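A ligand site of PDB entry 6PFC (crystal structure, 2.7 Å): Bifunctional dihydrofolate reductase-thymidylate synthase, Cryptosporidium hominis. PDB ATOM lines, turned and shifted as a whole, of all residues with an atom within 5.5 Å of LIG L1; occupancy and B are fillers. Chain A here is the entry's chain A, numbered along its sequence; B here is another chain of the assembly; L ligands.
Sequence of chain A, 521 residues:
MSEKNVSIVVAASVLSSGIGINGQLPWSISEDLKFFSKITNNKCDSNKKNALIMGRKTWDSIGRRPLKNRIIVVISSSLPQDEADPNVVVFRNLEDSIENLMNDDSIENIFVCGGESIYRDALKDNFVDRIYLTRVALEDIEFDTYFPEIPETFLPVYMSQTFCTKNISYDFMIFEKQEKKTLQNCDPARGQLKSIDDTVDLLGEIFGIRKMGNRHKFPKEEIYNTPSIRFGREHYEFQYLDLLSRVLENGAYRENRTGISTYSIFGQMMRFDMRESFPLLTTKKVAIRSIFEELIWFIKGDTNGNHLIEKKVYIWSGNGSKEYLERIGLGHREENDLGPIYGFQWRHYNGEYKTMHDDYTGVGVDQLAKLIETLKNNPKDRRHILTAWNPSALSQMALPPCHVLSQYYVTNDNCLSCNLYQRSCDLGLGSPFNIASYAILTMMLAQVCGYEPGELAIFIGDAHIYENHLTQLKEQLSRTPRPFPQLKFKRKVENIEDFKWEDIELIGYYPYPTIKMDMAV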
ATOM      1  N   ARG A 257      -1.273 -22.986  16.542  1.00  0.00           N
ATOM      2  CA  ARG A 257      -1.270 -21.803  15.687  1.00  0.00           C
ATOM      3  C   ARG A 257      -0.917 -20.526  16.448  1.00  0.00           C
ATOM      4  O   ARG A 257      -0.510 -19.548  15.819  1.00  0.00           O
ATOM      5  CB  ARG A 257      -2.642 -21.645  15.027  1.00  0.00           C
ATOM      6  CG  ARG A 257      -3.795 -21.546  16.016  1.00  0.00           C
ATOM      7  CD  ARG A 257      -5.094 -21.184  15.330  1.00  0.00           C
ATOM      8  NE  ARG A 257      -6.175 -20.975  16.289  1.00  0.00           N
ATOM      9  CZ  ARG A 257      -6.391 -19.820  16.913  1.00  0.00           C
ATOM     10  NH1 ARG A 257      -5.609 -18.782  16.684  1.00  0.00           N
ATOM     11  NH2 ARG A 257      -7.393 -19.719  17.781  1.00  0.00           N
ATOM     12  N   GLU A 294     -23.289 -13.937  25.067  1.00  0.00           N
ATOM     13  CA  GLU A 294     -22.770 -14.643  23.906  1.00  0.00           C
ATOM     14  C   GLU A 294     -23.775 -15.655  23.368  1.00  0.00           C
ATOM     15  O   GLU A 294     -23.908 -15.828  22.154  1.00  0.00           O
ATOM     16  CB  GLU A 294     -21.446 -15.326  24.260  1.00  0.00           C
ATOM     17  CG  GLU A 294     -20.784 -16.065  23.113  1.00  0.00           C
ATOM     18  CD  GLU A 294     -19.747 -17.076  23.588  1.00  0.00           C
ATOM     19  OE1 GLU A 294     -19.981 -17.707  24.639  1.00  0.00           O
ATOM     20  OE2 GLU A 294     -18.711 -17.245  22.907  1.00  0.00           O
ATOM     21  N   TRP A 316     -14.720 -11.811  22.304  1.00  0.00           N
ATOM     22  CA  TRP A 316     -14.441 -11.978  20.879  1.00  0.00           C
ATOM     23  C   TRP A 316     -13.631 -10.819  20.311  1.00  0.00           C
ATOM     24  O   TRP A 316     -13.563 -10.664  19.093  1.00  0.00           O
ATOM     25  CB  TRP A 316     -15.746 -12.146  20.106  1.00  0.00           C
ATOM     26  CG  TRP A 316     -16.366 -13.504  20.248  1.00  0.00           C
ATOM     27  CD1 TRP A 316     -17.366 -13.863  21.112  1.00  0.00           C
ATOM     28  CD2 TRP A 316     -16.035 -14.676  19.503  1.00  0.00           C
ATOM     29  NE1 TRP A 316     -17.666 -15.191  20.940  1.00  0.00           N
ATOM     30  CE2 TRP A 316     -16.874 -15.711  19.959  1.00  0.00           C
ATOM     31  CE3 TRP A 316     -15.123 -14.952  18.482  1.00  0.00           C
ATOM     32  CZ2 TRP A 316     -16.810 -17.009  19.450  1.00  0.00           C
ATOM     33  CZ3 TRP A 316     -15.060 -16.233  17.971  1.00  0.00           C
ATOM     34  CH2 TRP A 316     -15.907 -17.247  18.452  1.00  0.00           C
ATOM     35  N   TYR A 342     -20.871 -19.367  14.686  1.00  0.00           N
ATOM     36  CA  TYR A 342     -22.008 -19.729  15.526  1.00  0.00           C
ATOM     37  C   TYR A 342     -23.126 -18.708  15.382  1.00  0.00           C
ATOM     38  O   TYR A 342     -22.891 -17.504  15.387  1.00  0.00           O
ATOM     39  CB  TYR A 342     -21.587 -19.832  16.993  1.00  0.00           C
ATOM     40  CG  TYR A 342     -20.235 -20.450  17.259  1.00  0.00           C
ATOM     41  CD1 TYR A 342     -20.040 -21.823  17.165  1.00  0.00           C
ATOM     42  CD2 TYR A 342     -19.166 -19.658  17.649  1.00  0.00           C
ATOM     43  CE1 TYR A 342     -18.800 -22.382  17.421  1.00  0.00           C
ATOM     44  CE2 TYR A 342     -17.932 -20.211  17.911  1.00  0.00           C
ATOM     45  CZ  TYR A 342     -17.755 -21.575  17.803  1.00  0.00           C
ATOM     46  OH  TYR A 342     -16.514 -22.104  18.064  1.00  0.00           O
ATOM     47  N   LEU A 399     -12.795 -17.838  12.955  1.00  0.00           N
ATOM     48  CA  LEU A 399     -12.360 -18.961  13.785  1.00  0.00           C
ATOM     49  C   LEU A 399     -13.316 -20.133  13.568  1.00  0.00           C
ATOM     50  O   LEU A 399     -14.536 -19.979  13.741  1.00  0.00           O
ATOM     51  CB  LEU A 399     -12.321 -18.554  15.256  1.00  0.00           C
ATOM     52  CG  LEU A 399     -11.597 -19.515  16.214  1.00  0.00           C
ATOM     53  CD1 LEU A 399     -10.128 -19.627  15.846  1.00  0.00           C
ATOM     54  CD2 LEU A 399     -11.765 -19.057  17.650  1.00  0.00           C
ATOM     55  N   PRO A 400     -12.807 -21.303  13.197  1.00  0.00           N
ATOM     56  CA  PRO A 400     -13.676 -22.475  13.004  1.00  0.00           C
ATOM     57  C   PRO A 400     -14.375 -22.849  14.294  1.00  0.00           C
ATOM     58  O   PRO A 400     -13.899 -22.526  15.393  1.00  0.00           O
ATOM     59  CB  PRO A 400     -12.692 -23.566  12.550  1.00  0.00           C
ATOM     60  CG  PRO A 400     -11.572 -22.804  11.931  1.00  0.00           C
ATOM     61  CD  PRO A 400     -11.422 -21.567  12.758  1.00  0.00           C
ATOM     62  N   CYS A 402     -15.517 -24.422  17.633  1.00  0.00           N
ATOM     63  CA  CYS A 402     -14.937 -25.286  18.657  1.00  0.00           C
ATOM     64  C   CYS A 402     -15.974 -26.259  19.199  1.00  0.00           C
ATOM     65  O   CYS A 402     -15.789 -27.477  19.099  1.00  0.00           O
ATOM     66  CB  CYS A 402     -14.348 -24.425  19.784  1.00  0.00           C
ATOM     67  SG  CYS A 402     -12.934 -23.452  19.259  1.00  0.00           S
ATOM     68  N   HIS A 403     -17.067 -25.741  19.757  1.00  0.00           N
ATOM     69  CA  HIS A 403     -18.228 -26.588  20.049  1.00  0.00           C
ATOM     70  C   HIS A 403     -18.914 -26.878  18.732  1.00  0.00           C
ATOM     71  O   HIS A 403     -19.688 -26.066  18.220  1.00  0.00           O
ATOM     72  CB  HIS A 403     -19.158 -25.924  21.063  1.00  0.00           C
ATOM     73  CG  HIS A 403     -19.412 -24.468  20.821  1.00  0.00           C
ATOM     74  ND1 HIS A 403     -20.630 -23.994  20.396  1.00  0.00           N
ATOM     75  CD2 HIS A 403     -18.618 -23.385  20.974  1.00  0.00           C
ATOM     76  CE1 HIS A 403     -20.573 -22.673  20.278  1.00  0.00           C
ATOM     77  NE2 HIS A 403     -19.360 -22.283  20.623  1.00  0.00           N
ATOM     78  N   GLN A 422     -16.910 -31.187  21.299  1.00  0.00           N
ATOM     79  CA  GLN A 422     -16.036 -30.018  21.198  1.00  0.00           C
ATOM     80  C   GLN A 422     -14.675 -30.470  20.663  1.00  0.00           C
ATOM     81  O   GLN A 422     -14.001 -31.283  21.295  1.00  0.00           O
ATOM     82  CB  GLN A 422     -15.890 -29.337  22.555  1.00  0.00           C
ATOM     83  CG  GLN A 422     -15.117 -28.029  22.521  1.00  0.00           C
ATOM     84  CD  GLN A 422     -15.111 -27.336  23.874  1.00  0.00           C
ATOM     85  OE1 GLN A 422     -15.502 -27.909  24.882  1.00  0.00           O
ATOM     86  NE2 GLN A 422     -14.669 -26.082  23.887  1.00  0.00           N
ATOM     87  N   ARG A 423     -14.295 -29.929  19.502  1.00  0.00           N
ATOM     88  CA  ARG A 423     -13.057 -30.383  18.859  1.00  0.00           C
ATOM     89  C   ARG A 423     -11.825 -29.899  19.611  1.00  0.00           C
ATOM     90  O   ARG A 423     -10.820 -30.612  19.695  1.00  0.00           O
ATOM     91  CB  ARG A 423     -13.017 -29.904  17.403  1.00  0.00           C
ATOM     92  CG  ARG A 423     -12.987 -28.398  17.241  1.00  0.00           C
ATOM     93  CD  ARG A 423     -12.454 -27.998  15.880  1.00  0.00           C
ATOM     94  NE  ARG A 423     -12.379 -26.548  15.722  1.00  0.00           N
ATOM     95  CZ  ARG A 423     -11.334 -25.814  16.076  1.00  0.00           C
ATOM     96  NH1 ARG A 423     -10.262 -26.390  16.613  1.00  0.00           N
ATOM     97  NH2 ARG A 423     -11.356 -24.497  15.907  1.00  0.00           N
ATOM     98  N   SER A 424     -11.880 -28.684  20.155  1.00  0.00           N
ATOM     99  CA  SER A 424     -10.755 -28.093  20.865  1.00  0.00           C
ATOM    100  C   SER A 424     -11.294 -27.363  22.091  1.00  0.00           C
ATOM    101  O   SER A 424     -12.288 -26.645  21.995  1.00  0.00           O
ATOM    102  CB  SER A 424      -9.957 -27.134  19.970  1.00  0.00           C
ATOM    103  OG  SER A 424      -8.799 -26.653  20.636  1.00  0.00           O
ATOM    104  N   CYS A 425     -10.624 -27.551  23.224  1.00  0.00           N
ATOM    105  CA  CYS A 425     -11.146 -27.092  24.510  1.00  0.00           C
ATOM    106  C   CYS A 425     -10.042 -26.378  25.281  1.00  0.00           C
ATOM    107  O   CYS A 425      -9.128 -27.027  25.797  1.00  0.00           O
ATOM    108  CB  CYS A 425     -11.702 -28.262  25.320  1.00  0.00           C
ATOM    109  SG  CYS A 425     -12.511 -27.777  26.847  1.00  0.00           S
ATOM    110  N   ASP A 426     -10.143 -25.054  25.370  1.00  0.00           N
ATOM    111  CA  ASP A 426      -9.307 -24.265  26.264  1.00  0.00           C
ATOM    112  C   ASP A 426      -9.856 -24.454  27.685  1.00  0.00           C
ATOM    113  O   ASP A 426     -10.850 -23.839  28.059  1.00  0.00           O
ATOM    114  CB  ASP A 426      -9.306 -22.797  25.855  1.00  0.00           C
ATOM    115  CG  ASP A 426      -8.343 -21.955  26.675  1.00  0.00           C
ATOM    116  OD1 ASP A 426      -7.732 -22.477  27.631  1.00  0.00           O
ATOM    117  OD2 ASP A 426      -8.201 -20.756  26.352  1.00  0.00           O
ATOM    118  N   GLY A 430     -12.157 -21.320  27.840  1.00  0.00           N
ATOM    119  CA  GLY A 430     -13.310 -21.734  27.058  1.00  0.00           C
ATOM    120  C   GLY A 430     -14.202 -22.728  27.760  1.00  0.00           C
ATOM    121  O   GLY A 430     -15.429 -22.626  27.708  1.00  0.00           O
ATOM    122  N   SER A 431     -13.601 -23.717  28.444  1.00  0.00           N
ATOM    123  CA  SER A 431     -14.386 -24.798  29.024  1.00  0.00           C
ATOM    124  C   SER A 431     -15.425 -24.318  30.037  1.00  0.00           C
ATOM    125  O   SER A 431     -16.590 -24.739  29.931  1.00  0.00           O
ATOM    126  CB  SER A 431     -13.446 -25.847  29.632  1.00  0.00           C
ATOM    127  OG  SER A 431     -14.160 -27.025  29.977  1.00  0.00           O
ATOM    128  N   ASN A 434     -18.240 -22.876  28.025  1.00  0.00           N
ATOM    129  CA  ASN A 434     -19.014 -23.845  27.250  1.00  0.00           C
ATOM    130  C   ASN A 434     -19.963 -24.649  28.129  1.00  0.00           C
ATOM    131  O   ASN A 434     -21.074 -24.987  27.703  1.00  0.00           O
ATOM    132  CB  ASN A 434     -18.068 -24.775  26.486  1.00  0.00           C
ATOM    133  CG  ASN A 434     -17.287 -24.055  25.407  1.00  0.00           C
ATOM    134  OD1 ASN A 434     -16.059 -24.109  25.380  1.00  0.00           O
ATOM    135  ND2 ASN A 434     -17.999 -23.377  24.515  1.00  0.00           N
ATOM    136  N   HIS A 464      -6.810 -29.308  26.284  1.00  0.00           N
ATOM    137  CA  HIS A 464      -5.471 -28.766  26.469  1.00  0.00           C
ATOM    138  C   HIS A 464      -5.492 -27.629  27.474  1.00  0.00           C
ATOM    139  O   HIS A 464      -6.536 -27.049  27.772  1.00  0.00           O
ATOM    140  CB  HIS A 464      -4.887 -28.291  25.135  1.00  0.00           C
ATOM    141  CG  HIS A 464      -5.774 -27.338  24.391  1.00  0.00           C
ATOM    142  ND1 HIS A 464      -5.886 -26.007  24.720  1.00  0.00           N
ATOM    143  CD2 HIS A 464      -6.605 -27.542  23.333  1.00  0.00           C
ATOM    144  CE1 HIS A 464      -6.740 -25.424  23.896  1.00  0.00           C
ATOM    145  NE2 HIS A 464      -7.184 -26.332  23.044  1.00  0.00           N
ATOM    146  N   TYR A 466      -3.213 -24.090  28.248  1.00  0.00           N
ATOM    147  CA  TYR A 466      -2.170 -23.179  27.811  1.00  0.00           C
ATOM    148  C   TYR A 466      -1.139 -22.973  28.910  1.00  0.00           C
ATOM    149  O   TYR A 466      -1.474 -22.875  30.091  1.00  0.00           O
ATOM    150  CB  TYR A 466      -2.778 -21.841  27.388  1.00  0.00           C
ATOM    151  CG  TYR A 466      -3.493 -21.902  26.050  1.00  0.00           C
ATOM    152  CD1 TYR A 466      -4.821 -22.274  25.967  1.00  0.00           C
ATOM    153  CD2 TYR A 466      -2.815 -21.607  24.875  1.00  0.00           C
ATOM    154  CE1 TYR A 466      -5.477 -22.335  24.742  1.00  0.00           C
ATOM    155  CE2 TYR A 466      -3.450 -21.662  23.647  1.00  0.00           C
ATOM    156  CZ  TYR A 466      -4.772 -22.031  23.588  1.00  0.00           C
ATOM    157  OH  TYR A 466      -5.412 -22.097  22.367  1.00  0.00           O
ATOM    158  N   ARG B 382      -5.541 -28.719  15.132  1.00  0.00           N
ATOM    159  CA  ARG B 382      -6.680 -29.177  15.909  1.00  0.00           C
ATOM    160  C   ARG B 382      -7.981 -29.125  15.126  1.00  0.00           C
ATOM    161  O   ARG B 382      -9.054 -28.872  15.698  1.00  0.00           O
ATOM    162  CB  ARG B 382      -6.793 -28.357  17.200  1.00  0.00           C
ATOM    163  CG  ARG B 382      -5.577 -28.507  18.104  1.00  0.00           C
ATOM    164  CD  ARG B 382      -5.688 -27.684  19.372  1.00  0.00           C
ATOM    165  NE  ARG B 382      -5.567 -26.250  19.112  1.00  0.00           N
ATOM    166  CZ  ARG B 382      -5.108 -25.367  19.993  1.00  0.00           C
ATOM    167  NH1 ARG B 382      -4.704 -25.773  21.195  1.00  0.00           N
ATOM    168  NH2 ARG B 382      -5.031 -24.089  19.672  1.00  0.00           N
ATOM    169  N   ARG B 383      -7.924 -29.363  13.803  1.00  0.00           N
ATOM    170  CA  ARG B 383      -9.114 -29.278  12.973  1.00  0.00           C
ATOM    171  C   ARG B 383      -9.230 -30.445  11.999  1.00  0.00           C
ATOM    172  O   ARG B 383      -9.921 -30.318  10.979  1.00  0.00           O
ATOM    173  CB  ARG B 383      -9.122 -27.952  12.187  1.00  0.00           C
ATOM    174  CG  ARG B 383      -8.922 -26.716  13.035  1.00  0.00           C
ATOM    175  CD  ARG B 383      -8.980 -25.446  12.197  1.00  0.00           C
ATOM    176  NE  ARG B 383      -8.879 -24.245  13.030  1.00  0.00           N
ATOM    177  CZ  ARG B 383      -7.820 -23.438  13.046  1.00  0.00           C
ATOM    178  NH1 ARG B 383      -6.768 -23.705  12.285  1.00  0.00           N
ATOM    179  NH2 ARG B 383      -7.818 -22.376  13.830  1.00  0.00           N
HETATM  180  N1  LIG L   1     -12.060 -22.293  22.514  1.00  0.00           N
HETATM  181  C1  LIG L   1     -12.789 -23.110  23.316  1.00  0.00           C
HETATM  182  N2  LIG L   1     -14.124 -22.958  23.413  1.00  0.00           N
HETATM  183  C2  LIG L   1     -14.781 -22.008  22.711  1.00  0.00           C
HETATM  184  C3  LIG L   1     -14.035 -21.156  21.866  1.00  0.00           C
HETATM  185  C4  LIG L   1     -12.693 -21.322  21.795  1.00  0.00           C
HETATM  186  O1  LIG L   1     -12.286 -23.994  23.989  1.00  0.00           O
HETATM  187  O2  LIG L   1     -15.983 -21.891  22.813  1.00  0.00           O
HETATM  188  F1  LIG L   1     -14.632 -20.177  21.141  1.00  0.00           F
HETATM  189  C5  LIG L   1     -10.591 -22.348  22.318  1.00  0.00           C
HETATM  190  C6  LIG L   1     -10.033 -23.733  21.935  1.00  0.00           C
HETATM  191  C7  LIG L   1      -8.647 -23.327  21.402  1.00  0.00           C
HETATM  192  C8  LIG L   1      -8.968 -22.036  20.621  1.00  0.00           C
HETATM  193  O3  LIG L   1      -7.775 -23.020  22.482  1.00  0.00           O
HETATM  194  O4  LIG L   1     -10.233 -21.545  21.163  1.00  0.00           O
HETATM  195  C9  LIG L   1      -9.084 -22.294  19.112  1.00  0.00           C
HETATM  196  O5  LIG L   1      -8.934 -23.685  18.845  1.00  0.00           O
HETATM  197  P1  LIG L   1      -8.099 -23.840  17.478  1.00  0.00           P
HETATM  198  O6  LIG L   1      -7.781 -25.271  17.262  1.00  0.00           O
HETATM  199  O7  LIG L   1      -6.727 -23.007  17.601  1.00  0.00           O
HETATM  200  O8  LIG L   1      -8.951 -23.281  16.243  1.00  0.00           O
HETATM  201  O1  LG2 L   2     -11.633 -19.292  25.110  1.00  0.00           O
HETATM  202  C1  LG2 L   2     -13.092 -17.314  21.418  1.00  0.00           C
HETATM  203  C2  LG2 L   2     -14.246 -17.809  23.674  1.00  0.00           C
HETATM  204  C3  LG2 L   2     -14.242 -17.517  26.212  1.00  0.00           C
HETATM  205  C4  LG2 L   2     -13.818 -16.843  27.374  1.00  0.00           C
HETATM  206  C5  LG2 L   2     -12.948 -15.737  27.287  1.00  0.00           C
HETATM  207  C6  LG2 L   2     -12.500 -15.317  26.018  1.00  0.00           C
HETATM  208  C7  LG2 L   2     -12.933 -15.980  24.852  1.00  0.00           C
HETATM  209  C8  LG2 L   2     -12.468 -15.005  28.525  1.00  0.00           C
HETATM  210  C9  LG2 L   2     -12.938 -14.734  30.955  1.00  0.00           C
HETATM  211  C10 LG2 L   2     -13.099 -13.347  31.234  1.00  0.00           C
HETATM  212  C11 LG2 L   2     -12.485 -13.750  33.574  1.00  0.00           C
HETATM  213  C12 LG2 L   2     -12.542 -15.603  32.003  1.00  0.00           C
HETATM  214  C13 LG2 L   2     -11.271 -17.142  34.091  1.00  0.00           C
HETATM  215  C14 LG2 L   2     -13.532 -12.322  30.187  1.00  0.00           C
HETATM  216  C15 LG2 L   2     -14.932 -11.782  30.464  1.00  0.00           C
HETATM  217  C16 LG2 L   2     -11.043 -18.160  21.772  1.00  0.00           C
HETATM  218  C17 LG2 L   2     -12.875 -12.878  32.549  1.00  0.00           C
HETATM  219  C18 LG2 L   2     -12.310 -15.127  33.319  1.00  0.00           C
HETATM  220  C19 LG2 L   2     -11.774 -18.368  22.916  1.00  0.00           C
HETATM  221  C20 LG2 L   2     -11.089 -19.047  24.036  1.00  0.00           C
HETATM  222  C21 LG2 L   2      -9.159 -19.129  22.583  1.00  0.00           C
HETATM  223  C22 LG2 L   2     -13.085 -17.825  22.692  1.00  0.00           C
HETATM  224  C23 LG2 L   2     -13.803 -17.086  24.939  1.00  0.00           C
HETATM  225  N1  LG2 L   2      -9.719 -18.530  21.572  1.00  0.00           N
HETATM  226  N2  LG2 L   2      -9.804 -19.394  23.801  1.00  0.00           N
HETATM  227  N3  LG2 L   2     -11.848 -17.523  20.859  1.00  0.00           N
HETATM  228  N4  LG2 L   2      -7.855 -19.584  22.587  1.00  0.00           N
HETATM  229  N5  LG2 L   2     -13.160 -15.255  29.647  1.00  0.00           N
HETATM  230  O2  LG2 L   2     -11.505 -14.237  28.452  1.00  0.00           O
HETATM  231  O3  LG2 L   2     -11.927 -15.920  34.377  1.00  0.00           O
HETATM  232  O4  LG2 L   2     -15.264 -10.622  30.257  1.00  0.00           O
HETATM  233  O5  LG2 L   2     -15.758 -12.751  30.976  1.00  0.00           O
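An oxygen (O4) of LIG L1 lies close to a nitrogen (N4) of LG2 L2 (3.4 Å).
O of Pro 400 lies within hydrogen-bond range of NH2 of Arg 423, 3.3 Å away. The backbone carbonyl oxygen (O) of Asp 426 sits at hydrogen-bond distance from the backbone NH (N) of Ser 431 (2.8 Å). The guanidinium group of Arg 382 of chain B lies within hydrogen-bond range of a ring nitrogen (NE2) of His 464 (3.1 Å). A ring nitrogen (NE2) of His 464 is in hydrogen-bond range of the side-chain hydroxyl of Ser 424. The backbone NH of His 464 lies within hydrogen-bond range of the backbone carbonyl oxygen of Cys 425, at 3.3 Å. The side-chain amide oxygen of Asn 434 lies within hydrogen-bond range of the side-chain amide nitrogen of Gln 422. The backbone carbonyl oxygen of Ser 424 lies within hydrogen-bond range of the side-chain amide nitrogen of Gln 422 (3.1 Å). SG of Cys 425 lies close to OG of Ser 431 (3.6 Å).
The side-chain sulfur of Cys 402 lies close to a nitrogen (N1) of LIG L1, at 3.6 Å. Leu 399 touches LIG L1. His 403 touches LIG L1 (CD2 to O2, 3.5 Å). Cys 425 touches LIG L1 (CA to O1, 3.3 Å). Gly 430 touches LIG L1 (CA to N2, 3.9 Å). Hydrophobic or aromatic side chains within 4 Å of LIG L1: Leu 399, His 403, His 464 and Tyr 466. 15 residues have an atom within 4 Å of LIG L1: Arg 257, Leu 399, Cys 402, His 403, Gln 422, Arg 423, Ser 424, Cys 425, Asp 426, Gly 430, Asn 434, His 464, Tyr 466, Arg 382 of chain B and Arg 383 of chain B.
O7 of LIG L1 lies within salt-bridge range of NE of Arg 257, 2.5 Å away. The side-chain hydroxyl (OH) of Tyr 466 is in hydrogen-bond range of an oxygen (O3) of LIG L1 (2.5 Å). The guanidinium group (NH2) of Arg 423 lies within salt-bridge range of an oxygen (O8) of LIG L1. An oxygen (O1) of LIG L1 sits at hydrogen-bond distance from the backbone NH (N) of Asp 426 (2.8 Å). An oxygen (O8) of LIG L1 lies within salt-bridge range of the guanidinium group (NH2) of Arg 383 of chain B. O7 of LIG L1 is in salt-bridge range of NH2 of Arg 382 of chain B, 2.9 Å away. An oxygen (O3) of LIG L1 lies close to a ring nitrogen (NE2) of His 464 (3.4 Å). OD1 of Asn 434 is in hydrogen-bond range of N2 of LIG L1. NE2 of Gln 422 is in hydrogen-bond range of O1 of LIG L1, 3.2 Å away. O5 of LIG L1 sits close to OG of Ser 424, 3.5 Å away. N2 of LG2 L2 lies within hydrogen-bond range of OD2 of Asp 426 (3.3 Å). An oxygen (O1) of LG2 L2 lies within hydrogen-bond range of the backbone NH of Gly 430 (3.4 Å).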
